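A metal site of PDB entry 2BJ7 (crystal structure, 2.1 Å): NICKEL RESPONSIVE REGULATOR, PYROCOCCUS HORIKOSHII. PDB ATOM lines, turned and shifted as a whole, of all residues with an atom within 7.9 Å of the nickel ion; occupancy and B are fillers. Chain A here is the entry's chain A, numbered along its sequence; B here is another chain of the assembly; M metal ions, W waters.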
ATOM      1  N   ASN A  63      14.572  -8.631   8.482  1.00  0.00           N
ATOM      2  CA  ASN A  63      13.808  -7.870   9.450  1.00  0.00           C
ATOM      3  C   ASN A  63      12.421  -8.481   9.329  1.00  0.00           C
ATOM      4  O   ASN A  63      11.772  -8.328   8.296  1.00  0.00           O
ATOM      5  CB  ASN A  63      13.737  -6.402   9.054  1.00  0.00           C
ATOM      6  CG  ASN A  63      12.933  -5.588  10.044  1.00  0.00           C
ATOM      7  OD1 ASN A  63      11.858  -6.006  10.492  1.00  0.00           O
ATOM      8  ND2 ASN A  63      13.449  -4.416  10.399  1.00  0.00           N
ATOM      9  N   HIS A  64      11.959  -9.174  10.370  1.00  0.00           N
ATOM     10  CA  HIS A  64      10.661  -9.829  10.292  1.00  0.00           C
ATOM     11  C   HIS A  64       9.488  -8.876  10.159  1.00  0.00           C
ATOM     12  O   HIS A  64       8.384  -9.292   9.838  1.00  0.00           O
ATOM     13  CB  HIS A  64      10.434 -10.755  11.488  1.00  0.00           C
ATOM     14  CG  HIS A  64      10.207 -10.025  12.767  1.00  0.00           C
ATOM     15  ND1 HIS A  64      11.242  -9.673  13.620  1.00  0.00           N
ATOM     16  CD2 HIS A  64       9.074  -9.553  13.333  1.00  0.00           C
ATOM     17  CE1 HIS A  64      10.752  -9.014  14.650  1.00  0.00           C
ATOM     18  NE2 HIS A  64       9.442  -8.928  14.506  1.00  0.00           N
ATOM     19  N   ASP A  65       9.724  -7.595  10.422  1.00  0.00           N
ATOM     20  CA  ASP A  65       8.649  -6.607  10.311  1.00  0.00           C
ATOM     21  C   ASP A  65       8.613  -5.936   8.936  1.00  0.00           C
ATOM     22  O   ASP A  65       7.799  -5.061   8.702  1.00  0.00           O
ATOM     23  CB  ASP A  65       8.783  -5.541  11.401  1.00  0.00           C
ATOM     24  CG  ASP A  65       8.518  -6.094  12.785  1.00  0.00           C
ATOM     25  OD1 ASP A  65       7.479  -6.767  12.956  1.00  0.00           O
ATOM     26  OD2 ASP A  65       9.346  -5.867  13.700  1.00  0.00           O
ATOM     27  N   GLU A  66       9.495  -6.358   8.043  1.00  0.00           N
ATOM     28  CA  GLU A  66       9.555  -5.780   6.706  1.00  0.00           C
ATOM     29  C   GLU A  66       8.629  -6.497   5.733  1.00  0.00           C
ATOM     30  O   GLU A  66       8.610  -7.732   5.672  1.00  0.00           O
ATOM     31  CB  GLU A  66      10.989  -5.811   6.169  1.00  0.00           C
ATOM     32  CG  GLU A  66      11.177  -5.022   4.875  1.00  0.00           C
ATOM     33  CD  GLU A  66      12.616  -5.041   4.389  1.00  0.00           C
ATOM     34  OE1 GLU A  66      13.523  -4.676   5.164  1.00  0.00           O
ATOM     35  OE2 GLU A  66      12.839  -5.404   3.209  1.00  0.00           O
ATOM     36  N   VAL A  70       8.110 -12.626   6.150  1.00  0.00           N
ATOM     37  CA  VAL A  70       7.794 -13.744   7.027  1.00  0.00           C
ATOM     38  C   VAL A  70       6.764 -14.697   6.414  1.00  0.00           C
ATOM     39  O   VAL A  70       6.934 -15.916   6.471  1.00  0.00           O
ATOM     40  CB  VAL A  70       7.293 -13.257   8.411  1.00  0.00           C
ATOM     41  CG1 VAL A  70       6.743 -14.429   9.203  1.00  0.00           C
ATOM     42  CG2 VAL A  70       8.444 -12.636   9.190  1.00  0.00           C
ATOM     43  N   GLU A  94      15.366  -6.657  18.361  1.00  0.00           N
ATOM     44  CA  GLU A  94      13.950  -6.348  18.273  1.00  0.00           C
ATOM     45  C   GLU A  94      13.333  -6.624  16.905  1.00  0.00           C
ATOM     46  O   GLU A  94      12.180  -7.058  16.821  1.00  0.00           O
ATOM     47  CB  GLU A  94      13.729  -4.876  18.642  1.00  0.00           C
ATOM     48  CG  GLU A  94      12.274  -4.447  18.664  1.00  0.00           C
ATOM     49  CD  GLU A  94      12.102  -2.988  19.015  1.00  0.00           C
ATOM     50  OE1 GLU A  94      10.942  -2.521  19.085  1.00  0.00           O
ATOM     51  OE2 GLU A  94      13.130  -2.282  19.209  1.00  0.00           O
ATOM     52  N   HIS A  95      14.098  -6.415  15.837  1.00  0.00           N
ATOM     53  CA  HIS A  95      13.573  -6.607  14.495  1.00  0.00           C
ATOM     54  C   HIS A  95      14.211  -7.695  13.634  1.00  0.00           C
ATOM     55  O   HIS A  95      13.538  -8.320  12.811  1.00  0.00           O
ATOM     56  CB  HIS A  95      13.676  -5.293  13.703  1.00  0.00           C
ATOM     57  CG  HIS A  95      12.949  -4.145  14.331  1.00  0.00           C
ATOM     58  ND1 HIS A  95      11.568  -4.059  14.374  1.00  0.00           N
ATOM     59  CD2 HIS A  95      13.402  -3.036  14.956  1.00  0.00           C
ATOM     60  CE1 HIS A  95      11.218  -2.955  14.987  1.00  0.00           C
ATOM     61  NE2 HIS A  95      12.310  -2.311  15.361  1.00  0.00           N
ATOM     62  N   LYS B  71       2.710 -13.562  13.146  1.00  0.00           N
ATOM     63  CA  LYS B  71       3.196 -12.236  13.504  1.00  0.00           C
ATOM     64  C   LYS B  71       3.166 -12.051  15.013  1.00  0.00           C
ATOM     65  O   LYS B  71       4.033 -11.393  15.593  1.00  0.00           O
ATOM     66  CB  LYS B  71       2.337 -11.169  12.833  1.00  0.00           C
ATOM     67  CG  LYS B  71       2.835  -9.745  13.020  1.00  0.00           C
ATOM     68  CD  LYS B  71       1.948  -8.753  12.259  1.00  0.00           C
ATOM     69  CE  LYS B  71       2.503  -7.333  12.339  1.00  0.00           C
ATOM     70  NZ  LYS B  71       2.566  -6.838  13.747  1.00  0.00           N
ATOM     71  N   ALA B  72       2.155 -12.637  15.660  1.00  0.00           N
ATOM     72  CA  ALA B  72       2.018 -12.521  17.104  1.00  0.00           C
ATOM     73  C   ALA B  72       3.154 -13.273  17.809  1.00  0.00           C
ATOM     74  O   ALA B  72       3.721 -12.772  18.773  1.00  0.00           O
ATOM     75  CB  ALA B  72       0.647 -13.063  17.546  1.00  0.00           C
ATOM     76  N   LEU B  74       6.234 -14.048  16.717  1.00  0.00           N
ATOM     77  CA  LEU B  74       7.491 -13.332  16.536  1.00  0.00           C
ATOM     78  C   LEU B  74       7.609 -12.115  17.439  1.00  0.00           C
ATOM     79  O   LEU B  74       8.667 -11.875  18.031  1.00  0.00           O
ATOM     80  CB  LEU B  74       7.634 -12.897  15.080  1.00  0.00           C
ATOM     81  CG  LEU B  74       8.092 -13.985  14.115  1.00  0.00           C
ATOM     82  CD1 LEU B  74       7.903 -13.531  12.675  1.00  0.00           C
ATOM     83  CD2 LEU B  74       9.551 -14.312  14.395  1.00  0.00           C
ATOM     84  N   ASP B  75       6.536 -11.344  17.547  1.00  0.00           N
ATOM     85  CA  ASP B  75       6.551 -10.151  18.379  1.00  0.00           C
ATOM     86  C   ASP B  75       6.761 -10.505  19.841  1.00  0.00           C
ATOM     87  O   ASP B  75       7.521  -9.829  20.536  1.00  0.00           O
ATOM     88  CB  ASP B  75       5.258  -9.354  18.191  1.00  0.00           C
ATOM     89  CG  ASP B  75       5.245  -8.600  16.867  1.00  0.00           C
ATOM     90  OD1 ASP B  75       4.197  -8.027  16.503  1.00  0.00           O
ATOM     91  OD2 ASP B  75       6.296  -8.584  16.194  1.00  0.00           O
ATOM     92  N   LEU B  76       6.083 -11.547  20.305  1.00  0.00           N
ATOM     93  CA  LEU B  76       6.242 -11.976  21.684  1.00  0.00           C
ATOM     94  C   LEU B  76       7.685 -12.437  21.919  1.00  0.00           C
ATOM     95  O   LEU B  76       8.348 -11.971  22.846  1.00  0.00           O
ATOM     96  CB  LEU B  76       5.282 -13.119  22.014  1.00  0.00           C
ATOM     97  CG  LEU B  76       3.840 -12.700  22.289  1.00  0.00           C
ATOM     98  CD1 LEU B  76       2.954 -13.925  22.435  1.00  0.00           C
ATOM     99  CD2 LEU B  76       3.790 -11.857  23.553  1.00  0.00           C
ATOM    100  N   HIS B  78      10.457 -11.826  20.232  1.00  0.00           N
ATOM    101  CA  HIS B  78      11.462 -10.777  20.137  1.00  0.00           C
ATOM    102  C   HIS B  78      11.407  -9.842  21.340  1.00  0.00           C
ATOM    103  O   HIS B  78      12.324  -9.045  21.565  1.00  0.00           O
ATOM    104  CB  HIS B  78      11.287 -10.004  18.823  1.00  0.00           C
ATOM    105  CG  HIS B  78      11.995 -10.626  17.663  1.00  0.00           C
ATOM    106  ND1 HIS B  78      13.149 -10.088  17.124  1.00  0.00           N
ATOM    107  CD2 HIS B  78      11.765 -11.768  16.981  1.00  0.00           C
ATOM    108  CE1 HIS B  78      13.580 -10.873  16.157  1.00  0.00           C
ATOM    109  NE2 HIS B  78      12.761 -11.902  16.046  1.00  0.00           N
HETATM  110 NI    NI M   1       7.607  -7.352  14.962  1.00  0.00          NI
HETATM  111  O   HOH W   1       5.808  -8.563  13.657  1.00  0.00           O
HETATM  112  O   HOH W   2       9.155  -6.803  16.239  1.00  0.00           O
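Water W2 binds the nickel ion (2.1 Å). OD1 of Asp 65 binds the nickel ion (2.1 Å). The nickel ion is bound by OD2 of Asp 75 of chain B. NE2 of His 64 binds the nickel ion (2.5 Å). The nickel ion is bound by water W1 (2.5 Å). The nickel ion has five donor atoms within binding distance. Slightly farther from the nickel ion lies the side-chain carboxylate (OD2) of Asp 65 (2.6 Å).
Water W2 lies within hydrogen-bond range of the side-chain carboxylate (OD2) of Asp 65 and the backbone carbonyl oxygen (O) of Glu 94.
The nearest printed residue that does not touch the nickel ion is Glu 94 (4.9 Å).
The side-chain amino group of Lys 71 of chain B is in salt-bridge range of the side-chain carboxylate of Asp 75 of chain B (3.4 Å). The backbone carbonyl oxygen (O) of His 95 lies within hydrogen-bond range of a ring nitrogen (ND1) of His 64 (2.8 Å). The backbone NH (N) of Asp 65 is in hydrogen-bond range of the side-chain amide oxygen (OD1) of Asn 63 (2.7 Å). ND1 of His 95 sits at hydrogen-bond distance from OD2 of Asp 65 (2.9 Å).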
